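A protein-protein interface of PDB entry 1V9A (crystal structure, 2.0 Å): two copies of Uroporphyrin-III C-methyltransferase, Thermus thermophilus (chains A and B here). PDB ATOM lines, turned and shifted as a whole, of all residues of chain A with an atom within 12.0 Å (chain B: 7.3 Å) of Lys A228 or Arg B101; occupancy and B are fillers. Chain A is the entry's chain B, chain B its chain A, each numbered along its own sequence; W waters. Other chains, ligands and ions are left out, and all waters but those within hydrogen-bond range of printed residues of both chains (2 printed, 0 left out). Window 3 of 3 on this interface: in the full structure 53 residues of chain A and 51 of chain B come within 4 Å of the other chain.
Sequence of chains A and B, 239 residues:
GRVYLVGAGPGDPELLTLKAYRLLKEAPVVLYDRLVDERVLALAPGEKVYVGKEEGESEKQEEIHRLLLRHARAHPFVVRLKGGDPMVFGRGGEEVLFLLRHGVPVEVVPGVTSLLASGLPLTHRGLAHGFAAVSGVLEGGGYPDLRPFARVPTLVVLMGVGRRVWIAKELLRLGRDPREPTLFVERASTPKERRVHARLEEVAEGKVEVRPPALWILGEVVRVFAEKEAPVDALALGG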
ATOM      1  N   PRO A 121     -12.829   9.622 -30.005  1.00  0.00           N
ATOM      2  CA  PRO A 121     -11.969   9.684 -31.184  1.00  0.00           C
ATOM      3  C   PRO A 121     -10.985   8.518 -31.083  1.00  0.00           C
ATOM      4  O   PRO A 121     -10.038   8.579 -30.310  1.00  0.00           O
ATOM      5  CB  PRO A 121     -11.285  11.044 -31.036  1.00  0.00           C
ATOM      6  CG  PRO A 121     -11.110  11.157 -29.571  1.00  0.00           C
ATOM      7  CD  PRO A 121     -12.433  10.637 -29.006  1.00  0.00           C
ATOM      8  N   HIS A 124      -6.331  10.132 -32.513  1.00  0.00           N
ATOM      9  CA  HIS A 124      -6.198  11.481 -31.990  1.00  0.00           C
ATOM     10  C   HIS A 124      -4.715  11.829 -31.939  1.00  0.00           C
ATOM     11  O   HIS A 124      -3.874  11.016 -31.529  1.00  0.00           O
ATOM     12  CB  HIS A 124      -6.805  11.569 -30.585  1.00  0.00           C
ATOM     13  CG  HIS A 124      -6.908  12.964 -30.043  1.00  0.00           C
ATOM     14  ND1 HIS A 124      -7.877  13.856 -30.453  1.00  0.00           N
ATOM     15  CD2 HIS A 124      -6.193  13.602 -29.083  1.00  0.00           C
ATOM     16  CE1 HIS A 124      -7.759  14.978 -29.766  1.00  0.00           C
ATOM     17  NE2 HIS A 124      -6.746  14.850 -28.928  1.00  0.00           N
ATOM     18  N   ARG A 125      -4.412  13.037 -32.384  1.00  0.00           N
ATOM     19  CA  ARG A 125      -3.054  13.554 -32.412  1.00  0.00           C
ATOM     20  C   ARG A 125      -2.280  13.306 -31.116  1.00  0.00           C
ATOM     21  O   ARG A 125      -2.747  13.655 -30.039  1.00  0.00           O
ATOM     22  CB  ARG A 125      -3.123  15.046 -32.689  1.00  0.00           C
ATOM     23  CG  ARG A 125      -1.795  15.736 -32.788  1.00  0.00           C
ATOM     24  CD  ARG A 125      -1.971  17.194 -33.192  1.00  0.00           C
ATOM     25  NE  ARG A 125      -0.765  17.941 -32.865  1.00  0.00           N
ATOM     26  CZ  ARG A 125      -0.615  18.680 -31.770  1.00  0.00           C
ATOM     27  NH1 ARG A 125      -1.608  18.792 -30.894  1.00  0.00           N
ATOM     28  NH2 ARG A 125       0.541  19.291 -31.541  1.00  0.00           N
ATOM     29  N   GLY A 126      -1.104  12.690 -31.238  1.00  0.00           N
ATOM     30  CA  GLY A 126      -0.261  12.423 -30.083  1.00  0.00           C
ATOM     31  C   GLY A 126      -0.630  11.214 -29.246  1.00  0.00           C
ATOM     32  O   GLY A 126       0.131  10.807 -28.369  1.00  0.00           O
ATOM     33  N   LEU A 127      -1.795  10.628 -29.508  1.00  0.00           N
ATOM     34  CA  LEU A 127      -2.230   9.472 -28.737  1.00  0.00           C
ATOM     35  C   LEU A 127      -2.319   8.208 -29.584  1.00  0.00           C
ATOM     36  O   LEU A 127      -1.870   7.141 -29.167  1.00  0.00           O
ATOM     37  CB  LEU A 127      -3.593   9.749 -28.091  1.00  0.00           C
ATOM     38  CG  LEU A 127      -3.685  10.924 -27.111  1.00  0.00           C
ATOM     39  CD1 LEU A 127      -5.112  11.039 -26.602  1.00  0.00           C
ATOM     40  CD2 LEU A 127      -2.724  10.713 -25.943  1.00  0.00           C
ATOM     41  N   GLU A 220      -5.146   5.636 -24.453  1.00  0.00           N
ATOM     42  CA  GLU A 220      -5.267   6.974 -23.882  1.00  0.00           C
ATOM     43  C   GLU A 220      -6.473   7.783 -24.393  1.00  0.00           C
ATOM     44  O   GLU A 220      -7.011   8.602 -23.656  1.00  0.00           O
ATOM     45  CB  GLU A 220      -3.980   7.774 -24.116  1.00  0.00           C
ATOM     46  CG  GLU A 220      -2.846   7.473 -23.132  1.00  0.00           C
ATOM     47  CD  GLU A 220      -3.195   7.822 -21.696  1.00  0.00           C
ATOM     48  OE1 GLU A 220      -3.720   8.933 -21.461  1.00  0.00           O
ATOM     49  OE2 GLU A 220      -2.936   6.988 -20.800  1.00  0.00           O
ATOM     50  N   VAL A 221      -6.900   7.559 -25.638  1.00  0.00           N
ATOM     51  CA  VAL A 221      -8.056   8.292 -26.180  1.00  0.00           C
ATOM     52  C   VAL A 221      -9.312   8.305 -25.284  1.00  0.00           C
ATOM     53  O   VAL A 221     -10.121   9.225 -25.361  1.00  0.00           O
ATOM     54  CB  VAL A 221      -8.522   7.729 -27.566  1.00  0.00           C
ATOM     55  CG1 VAL A 221      -7.424   7.858 -28.601  1.00  0.00           C
ATOM     56  CG2 VAL A 221      -8.971   6.255 -27.411  1.00  0.00           C
ATOM     57  N   VAL A 222      -9.477   7.254 -24.489  1.00  0.00           N
ATOM     58  CA  VAL A 222     -10.598   7.064 -23.575  1.00  0.00           C
ATOM     59  C   VAL A 222     -10.839   8.311 -22.699  1.00  0.00           C
ATOM     60  O   VAL A 222     -11.974   8.657 -22.336  1.00  0.00           O
ATOM     61  CB  VAL A 222     -10.246   5.865 -22.652  1.00  0.00           C
ATOM     62  CG1 VAL A 222     -10.970   5.936 -21.336  1.00  0.00           C
ATOM     63  CG2 VAL A 222     -10.554   4.602 -23.382  1.00  0.00           C
ATOM     64  N   ARG A 223      -9.709   8.892 -22.370  1.00  0.00           N
ATOM     65  CA  ARG A 223      -9.471  10.015 -21.512  1.00  0.00           C
ATOM     66  C   ARG A 223      -9.462  11.424 -22.094  1.00  0.00           C
ATOM     67  O   ARG A 223      -9.453  12.396 -21.321  1.00  0.00           O
ATOM     68  CB  ARG A 223      -8.123   9.745 -20.908  1.00  0.00           C
ATOM     69  CG  ARG A 223      -7.743  10.157 -19.524  1.00  0.00           C
ATOM     70  CD  ARG A 223      -6.483   9.403 -19.461  1.00  0.00           C
ATOM     71  NE  ARG A 223      -6.191   8.992 -18.130  1.00  0.00           N
ATOM     72  CZ  ARG A 223      -5.079   8.403 -17.760  1.00  0.00           C
ATOM     73  NH1 ARG A 223      -4.107   8.113 -18.621  1.00  0.00           N
ATOM     74  NH2 ARG A 223      -4.954   8.137 -16.485  1.00  0.00           N
ATOM     75  N   VAL A 224      -9.500  11.546 -23.417  1.00  0.00           N
ATOM     76  CA  VAL A 224      -9.473  12.845 -24.067  1.00  0.00           C
ATOM     77  C   VAL A 224     -10.446  13.917 -23.612  1.00  0.00           C
ATOM     78  O   VAL A 224     -10.043  15.067 -23.431  1.00  0.00           O
ATOM     79  CB  VAL A 224      -9.604  12.728 -25.606  1.00  0.00           C
ATOM     80  CG1 VAL A 224      -8.415  11.973 -26.180  1.00  0.00           C
ATOM     81  CG2 VAL A 224     -10.892  12.047 -25.979  1.00  0.00           C
ATOM     82  N   PHE A 225     -11.718  13.576 -23.450  1.00  0.00           N
ATOM     83  CA  PHE A 225     -12.701  14.585 -23.060  1.00  0.00           C
ATOM     84  C   PHE A 225     -12.924  14.750 -21.550  1.00  0.00           C
ATOM     85  O   PHE A 225     -13.870  15.418 -21.132  1.00  0.00           O
ATOM     86  CB  PHE A 225     -14.041  14.292 -23.750  1.00  0.00           C
ATOM     87  CG  PHE A 225     -13.942  14.145 -25.241  1.00  0.00           C
ATOM     88  CD1 PHE A 225     -13.202  15.056 -25.993  1.00  0.00           C
ATOM     89  CD2 PHE A 225     -14.596  13.104 -25.901  1.00  0.00           C
ATOM     90  CE1 PHE A 225     -13.110  14.935 -27.389  1.00  0.00           C
ATOM     91  CE2 PHE A 225     -14.512  12.975 -27.296  1.00  0.00           C
ATOM     92  CZ  PHE A 225     -13.768  13.892 -28.038  1.00  0.00           C
ATOM     93  N   ALA A 226     -12.070  14.152 -20.730  1.00  0.00           N
ATOM     94  CA  ALA A 226     -12.237  14.274 -19.282  1.00  0.00           C
ATOM     95  C   ALA A 226     -11.729  15.626 -18.788  1.00  0.00           C
ATOM     96  O   ALA A 226     -10.653  16.070 -19.187  1.00  0.00           O
ATOM     97  CB  ALA A 226     -11.493  13.147 -18.560  1.00  0.00           C
ATOM     98  N   GLU A 227     -12.506  16.275 -17.921  1.00  0.00           N
ATOM     99  CA  GLU A 227     -12.114  17.568 -17.365  1.00  0.00           C
ATOM    100  C   GLU A 227     -10.768  17.452 -16.647  1.00  0.00           C
ATOM    101  O   GLU A 227     -10.358  16.365 -16.228  1.00  0.00           O
ATOM    102  CB  GLU A 227     -13.187  18.077 -16.391  1.00  0.00           C
ATOM    103  CG  GLU A 227     -14.463  18.572 -17.074  1.00  0.00           C
ATOM    104  CD  GLU A 227     -14.286  19.932 -17.737  1.00  0.00           C
ATOM    105  OE1 GLU A 227     -13.182  20.219 -18.245  1.00  0.00           O
ATOM    106  OE2 GLU A 227     -15.256  20.715 -17.760  1.00  0.00           O
ATOM    107  N   LYS A 228     -10.087  18.582 -16.512  1.00  0.00           N
ATOM    108  CA  LYS A 228      -8.785  18.634 -15.853  1.00  0.00           C
ATOM    109  C   LYS A 228      -8.899  18.705 -14.334  1.00  0.00           C
ATOM    110  O   LYS A 228      -8.266  17.932 -13.615  1.00  0.00           O
ATOM    111  CB  LYS A 228      -8.015  19.866 -16.321  1.00  0.00           C
ATOM    112  CG  LYS A 228      -7.751  19.930 -17.804  1.00  0.00           C
ATOM    113  CD  LYS A 228      -7.163  21.286 -18.170  1.00  0.00           C
ATOM    114  CE  LYS A 228      -5.931  21.131 -19.043  1.00  0.00           C
ATOM    115  NZ  LYS A 228      -6.210  20.246 -20.208  1.00  0.00           N
ATOM    116  N   GLU A 229      -9.703  19.651 -13.857  1.00  0.00           N
ATOM    117  CA  GLU A 229      -9.876  19.858 -12.427  1.00  0.00           C
ATOM    118  C   GLU A 229     -10.686  18.777 -11.702  1.00  0.00           C
ATOM    119  O   GLU A 229     -10.728  18.768 -10.472  1.00  0.00           O
ATOM    120  CB  GLU A 229     -10.500  21.240 -12.173  1.00  0.00           C
ATOM    121  CG  GLU A 229      -9.620  22.433 -12.580  1.00  0.00           C
ATOM    122  CD  GLU A 229      -8.364  22.575 -11.728  1.00  0.00           C
ATOM    123  OE1 GLU A 229      -8.464  22.428 -10.492  1.00  0.00           O
ATOM    124  OE2 GLU A 229      -7.281  22.848 -12.293  1.00  0.00           O
ATOM    125  N   ALA A 230     -11.313  17.869 -12.451  1.00  0.00           N
ATOM    126  CA  ALA A 230     -12.109  16.796 -11.842  1.00  0.00           C
ATOM    127  C   ALA A 230     -12.508  15.681 -12.822  1.00  0.00           C
ATOM    128  O   ALA A 230     -12.538  15.892 -14.035  1.00  0.00           O
ATOM    129  CB  ALA A 230     -13.362  17.387 -11.197  1.00  0.00           C
ATOM    130  N   PRO A 231     -12.818  14.476 -12.302  1.00  0.00           N
ATOM    131  CA  PRO A 231     -13.214  13.350 -13.157  1.00  0.00           C
ATOM    132  C   PRO A 231     -14.611  13.579 -13.727  1.00  0.00           C
ATOM    133  O   PRO A 231     -15.571  12.909 -13.336  1.00  0.00           O
ATOM    134  CB  PRO A 231     -13.169  12.166 -12.202  1.00  0.00           C
ATOM    135  CG  PRO A 231     -13.618  12.777 -10.918  1.00  0.00           C
ATOM    136  CD  PRO A 231     -12.824  14.072 -10.884  1.00  0.00           C
ATOM    137  N   VAL A 232     -14.712  14.529 -14.651  1.00  0.00           N
ATOM    138  CA  VAL A 232     -15.981  14.877 -15.273  1.00  0.00           C
ATOM    139  C   VAL A 232     -15.949  14.675 -16.787  1.00  0.00           C
ATOM    140  O   VAL A 232     -15.014  15.108 -17.457  1.00  0.00           O
ATOM    141  CB  VAL A 232     -16.343  16.352 -14.966  1.00  0.00           C
ATOM    142  CG1 VAL A 232     -17.581  16.772 -15.761  1.00  0.00           C
ATOM    143  CG2 VAL A 232     -16.585  16.524 -13.473  1.00  0.00           C
ATOM    144  N   ASP A 233     -16.980  14.012 -17.313  1.00  0.00           N
ATOM    145  CA  ASP A 233     -17.091  13.754 -18.750  1.00  0.00           C
ATOM    146  C   ASP A 233     -17.599  15.032 -19.423  1.00  0.00           C
ATOM    147  O   ASP A 233     -18.809  15.246 -19.537  1.00  0.00           O
ATOM    148  CB  ASP A 233     -18.082  12.609 -19.010  1.00  0.00           C
ATOM    149  CG  ASP A 233     -17.990  12.057 -20.431  1.00  0.00           C
ATOM    150  OD1 ASP A 233     -17.761  12.842 -21.378  1.00  0.00           O
ATOM    151  OD2 ASP A 233     -18.161  10.829 -20.602  1.00  0.00           O
ATOM    152  N   ALA A 234     -16.672  15.878 -19.866  1.00  0.00           N
ATOM    153  CA  ALA A 234     -17.037  17.139 -20.498  1.00  0.00           C
ATOM    154  C   ALA A 234     -18.063  16.973 -21.621  1.00  0.00           C
ATOM    155  O   ALA A 234     -18.970  17.792 -21.761  1.00  0.00           O
ATOM    156  CB  ALA A 234     -15.783  17.848 -21.022  1.00  0.00           C
ATOM    157  N   LEU A 235     -17.935  15.907 -22.404  1.00  0.00           N
ATOM    158  CA  LEU A 235     -18.859  15.669 -23.519  1.00  0.00           C
ATOM    159  C   LEU A 235     -20.205  15.048 -23.142  1.00  0.00           C
ATOM    160  O   LEU A 235     -21.179  15.180 -23.884  1.00  0.00           O
ATOM    161  CB  LEU A 235     -18.196  14.789 -24.583  1.00  0.00           C
ATOM    162  CG  LEU A 235     -19.072  14.437 -25.791  1.00  0.00           C
ATOM    163  CD1 LEU A 235     -19.350  15.687 -26.613  1.00  0.00           C
ATOM    164  CD2 LEU A 235     -18.376  13.400 -26.634  1.00  0.00           C
ATOM    165  N   ALA A 236     -20.261  14.349 -22.015  1.00  0.00           N
ATOM    166  CA  ALA A 236     -21.519  13.748 -21.584  1.00  0.00           C
ATOM    167  C   ALA A 236     -22.393  14.865 -21.037  1.00  0.00           C
ATOM    168  O   ALA A 236     -23.620  14.831 -21.127  1.00  0.00           O
ATOM    169  CB  ALA A 236     -21.264  12.697 -20.502  1.00  0.00           C
ATOM    170  N   LEU A 237     -21.731  15.872 -20.478  1.00  0.00           N
ATOM    171  CA  LEU A 237     -22.399  17.031 -19.894  1.00  0.00           C
ATOM    172  C   LEU A 237     -22.171  18.291 -20.731  1.00  0.00           C
ATOM    173  O   LEU A 237     -22.291  19.363 -20.150  1.00  0.00           O
ATOM    174  CB  LEU A 237     -21.867  17.259 -18.482  1.00  0.00           C
ATOM    175  CG  LEU A 237     -22.173  16.151 -17.482  1.00  0.00           C
ATOM    176  CD1 LEU A 237     -21.328  16.323 -16.235  1.00  0.00           C
ATOM    177  CD2 LEU A 237     -23.656  16.167 -17.153  1.00  0.00           C
ATOM    178  N   GLU B  94      -9.886  16.587 -31.866  1.00  0.00           N
ATOM    179  CA  GLU B  94      -9.324  17.911 -31.579  1.00  0.00           C
ATOM    180  C   GLU B  94     -10.401  18.984 -31.684  1.00  0.00           C
ATOM    181  O   GLU B  94     -10.419  19.945 -30.912  1.00  0.00           O
ATOM    182  CB  GLU B  94      -8.202  18.247 -32.554  1.00  0.00           C
ATOM    183  CG  GLU B  94      -7.008  17.325 -32.515  1.00  0.00           C
ATOM    184  CD  GLU B  94      -5.999  17.672 -33.598  1.00  0.00           C
ATOM    185  OE1 GLU B  94      -5.452  18.796 -33.568  1.00  0.00           O
ATOM    186  OE2 GLU B  94      -5.759  16.826 -34.486  1.00  0.00           O
ATOM    187  N   GLU B  95     -11.294  18.820 -32.650  1.00  0.00           N
ATOM    188  CA  GLU B  95     -12.370  19.777 -32.844  1.00  0.00           C
ATOM    189  C   GLU B  95     -13.335  19.742 -31.664  1.00  0.00           C
ATOM    190  O   GLU B  95     -13.743  20.780 -31.139  1.00  0.00           O
ATOM    191  CB  GLU B  95     -13.101  19.469 -34.147  1.00  0.00           C
ATOM    192  CG  GLU B  95     -12.369  19.925 -35.396  1.00  0.00           C
ATOM    193  CD  GLU B  95     -13.145  19.605 -36.653  1.00  0.00           C
ATOM    194  OE1 GLU B  95     -14.393  19.623 -36.591  1.00  0.00           O
ATOM    195  OE2 GLU B  95     -12.518  19.340 -37.702  1.00  0.00           O
ATOM    196  N   VAL B  96     -13.705  18.542 -31.237  1.00  0.00           N
ATOM    197  CA  VAL B  96     -14.618  18.422 -30.121  1.00  0.00           C
ATOM    198  C   VAL B  96     -13.970  18.980 -28.846  1.00  0.00           C
ATOM    199  O   VAL B  96     -14.610  19.715 -28.080  1.00  0.00           O
ATOM    200  CB  VAL B  96     -15.040  16.949 -29.896  1.00  0.00           C
ATOM    201  CG1 VAL B  96     -15.779  16.811 -28.577  1.00  0.00           C
ATOM    202  CG2 VAL B  96     -15.954  16.498 -31.034  1.00  0.00           C
ATOM    203  N   LEU B  97     -12.705  18.637 -28.627  1.00  0.00           N
ATOM    204  CA  LEU B  97     -11.977  19.097 -27.444  1.00  0.00           C
ATOM    205  C   LEU B  97     -11.972  20.625 -27.372  1.00  0.00           C
ATOM    206  O   LEU B  97     -12.296  21.226 -26.340  1.00  0.00           O
ATOM    207  CB  LEU B  97     -10.535  18.585 -27.486  1.00  0.00           C
ATOM    208  CG  LEU B  97      -9.692  18.824 -26.234  1.00  0.00           C
ATOM    209  CD1 LEU B  97     -10.421  18.284 -25.011  1.00  0.00           C
ATOM    210  CD2 LEU B  97      -8.342  18.145 -26.392  1.00  0.00           C
ATOM    211  N   PHE B  98     -11.587  21.251 -28.477  1.00  0.00           N
ATOM    212  CA  PHE B  98     -11.546  22.701 -28.547  1.00  0.00           C
ATOM    213  C   PHE B  98     -12.883  23.331 -28.159  1.00  0.00           C
ATOM    214  O   PHE B  98     -12.938  24.247 -27.331  1.00  0.00           O
ATOM    215  CB  PHE B  98     -11.150  23.140 -29.964  1.00  0.00           C
ATOM    216  CG  PHE B  98     -11.190  24.631 -30.170  1.00  0.00           C
ATOM    217  CD1 PHE B  98     -12.360  25.254 -30.581  1.00  0.00           C
ATOM    218  CD2 PHE B  98     -10.061  25.414 -29.942  1.00  0.00           C
ATOM    219  CE1 PHE B  98     -12.412  26.634 -30.766  1.00  0.00           C
ATOM    220  CE2 PHE B  98     -10.103  26.796 -30.121  1.00  0.00           C
ATOM    221  CZ  PHE B  98     -11.283  27.403 -30.535  1.00  0.00           C
ATOM    222  N   LEU B  99     -13.961  22.835 -28.757  1.00  0.00           N
ATOM    223  CA  LEU B  99     -15.289  23.369 -28.487  1.00  0.00           C
ATOM    224  C   LEU B  99     -15.699  23.213 -27.023  1.00  0.00           C
ATOM    225  O   LEU B  99     -16.247  24.146 -26.427  1.00  0.00           O
ATOM    226  CB  LEU B  99     -16.312  22.701 -29.415  1.00  0.00           C
ATOM    227  CG  LEU B  99     -16.076  23.005 -30.902  1.00  0.00           C
ATOM    228  CD1 LEU B  99     -16.878  22.040 -31.777  1.00  0.00           C
ATOM    229  CD2 LEU B  99     -16.488  24.450 -31.189  1.00  0.00           C
ATOM    230  N   LEU B 100     -15.432  22.047 -26.439  1.00  0.00           N
ATOM    231  CA  LEU B 100     -15.790  21.822 -25.037  1.00  0.00           C
ATOM    232  C   LEU B 100     -15.057  22.820 -24.147  1.00  0.00           C
ATOM    233  O   LEU B 100     -15.656  23.423 -23.266  1.00  0.00           O
ATOM    234  CB  LEU B 100     -15.439  20.395 -24.617  1.00  0.00           C
ATOM    235  CG  LEU B 100     -16.194  19.321 -25.403  1.00  0.00           C
ATOM    236  CD1 LEU B 100     -15.950  17.969 -24.773  1.00  0.00           C
ATOM    237  CD2 LEU B 100     -17.679  19.636 -25.408  1.00  0.00           C
ATOM    238  N   ARG B 101     -13.764  22.991 -24.393  1.00  0.00           N
ATOM    239  CA  ARG B 101     -12.947  23.916 -23.620  1.00  0.00           C
ATOM    240  C   ARG B 101     -13.473  25.347 -23.722  1.00  0.00           C
ATOM    241  O   ARG B 101     -13.298  26.147 -22.806  1.00  0.00           O
ATOM    242  CB  ARG B 101     -11.490  23.844 -24.089  1.00  0.00           C
ATOM    243  CG  ARG B 101     -10.807  22.538 -23.681  1.00  0.00           C
ATOM    244  CD  ARG B 101      -9.425  22.409 -24.286  1.00  0.00           C
ATOM    245  NE  ARG B 101      -8.681  21.296 -23.703  1.00  0.00           N
ATOM    246  CZ  ARG B 101      -7.513  20.857 -24.160  1.00  0.00           C
ATOM    247  NH1 ARG B 101      -6.955  21.437 -25.216  1.00  0.00           N
ATOM    248  NH2 ARG B 101      -6.900  19.843 -23.559  1.00  0.00           N
ATOM    249  N   HIS B 102     -14.126  25.672 -24.831  1.00  0.00           N
ATOM    250  CA  HIS B 102     -14.675  27.011 -24.990  1.00  0.00           C
ATOM    251  C   HIS B 102     -16.144  27.048 -24.606  1.00  0.00           C
ATOM    252  O   HIS B 102     -16.859  28.000 -24.899  1.00  0.00           O
ATOM    253  CB  HIS B 102     -14.459  27.499 -26.415  1.00  0.00           C
ATOM    254  CG  HIS B 102     -13.028  27.787 -26.722  1.00  0.00           C
ATOM    255  ND1 HIS B 102     -12.493  29.054 -26.642  1.00  0.00           N
ATOM    256  CD2 HIS B 102     -11.996  26.960 -27.014  1.00  0.00           C
ATOM    257  CE1 HIS B 102     -11.191  28.996 -26.869  1.00  0.00           C
ATOM    258  NE2 HIS B 102     -10.865  27.736 -27.097  1.00  0.00           N
ATOM    259  N   GLY B 103     -16.590  25.995 -23.936  1.00  0.00           N
ATOM    260  CA  GLY B 103     -17.964  25.950 -23.476  1.00  0.00           C
ATOM    261  C   GLY B 103     -19.048  25.810 -24.518  1.00  0.00           C
ATOM    262  O   GLY B 103     -20.194  26.206 -24.271  1.00  0.00           O
ATOM    263  N   VAL B 104     -18.705  25.251 -25.675  1.00  0.00           N
ATOM    264  CA  VAL B 104     -19.693  25.042 -26.736  1.00  0.00           C
ATOM    265  C   VAL B 104     -20.199  23.605 -26.645  1.00  0.00           C
ATOM    266  O   VAL B 104     -19.419  22.664 -26.752  1.00  0.00           O
ATOM    267  CB  VAL B 104     -19.072  25.238 -28.127  1.00  0.00           C
ATOM    268  CG1 VAL B 104     -20.082  24.867 -29.206  1.00  0.00           C
ATOM    269  CG2 VAL B 104     -18.625  26.666 -28.287  1.00  0.00           C
HETATM  270  O   HOH W   1      -6.199  14.214 -34.337  1.00  0.00           O
HETATM  271  O   HOH W   2      -8.828  13.917 -33.131  1.00  0.00           O
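Of the printed residues of chain B, Arg A125 touches Glu B94 (3.7 Å). Of chain B, only Arg B101 comes within 4 Å of Lys A228. Of the printed residues of chain B, Ala A234 touches Leu B100. Leu B97 touches just these residues of chain A: Val A224 (3.6 Å) and Phe A225 (3.9 Å). Phe B98 touches none of the printed residues of chain A. Of chain A, only Ala A234 (3.8 Å) and Leu A235 (3.7 Å) come within 4 Å of Leu B100. Of chain A, only Lys A228 comes within 4 Å of Arg B101. No residue of chain A comes within 4 Å of His B102. The nearest residue of chain B that does not touch Lys A228 is Leu B97 (6.7 Å). The nearest printed residue of chain A that does not touch Glu B94 is Phe A225 (5.8 Å).
The guanidinium group of Arg B101 lies close to the side-chain amino group of Lys A228, at 3.4 Å.
Water W1 bridges OE2 of Glu B94 (2.7 Å) and N of Arg A125 (2.9 Å). Water W2 lies within hydrogen-bond range of a ring nitrogen (ND1) of His A124 (2.8 Å) and the backbone NH of Glu B94 (3.1 Å).
Of the 23 printed residues of chain A, 7 touch a printed residue of chain B. Hydrophobic or aromatic side chains of chain A within 4 Å of the printed part of chain B: His A124, Phe A225, Ala A234 and Leu A235. Of the 11 printed residues of chain B, 5 touch a printed residue of chain A. Printed residues of chain B that touch a printed residue of chain A: Glu B94, Val B96, Leu B97, Leu B100 and Arg B101. Hydrophobic or aromatic side chains of chain B that line the printed part of chain A: Val B96, Leu B97 and Leu B100. Among the printed residues, no Asp or Glu carboxylate lies within 4 Å of a Lys or Arg side-chain nitrogen of the other chain.
His A124 touches Glu B94. CB of Arg A125 touches OE2 of Glu B94, at 3.7 Å. Val A224 touches Leu B97. CE1 of Phe A225 touches CG1 of Val B96 (3.5 Å). CE1 of Phe A225 touches N of Leu B97, 3.9 Å away. Ala A234 touches Leu B100. N of Leu A235 touches CD1 of Leu B100, at 3.7 Å.
The backbone carbonyl oxygen (O) of Phe A225 sits close to the backbone NH (N) of Ala A234. N of Leu A235 lies close to OD1 of Asp A233.
No position is printed for both chains. Of the 8 pairs that touch across the chains among the printed residues, none has its exchanged pair printed and touching as well.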
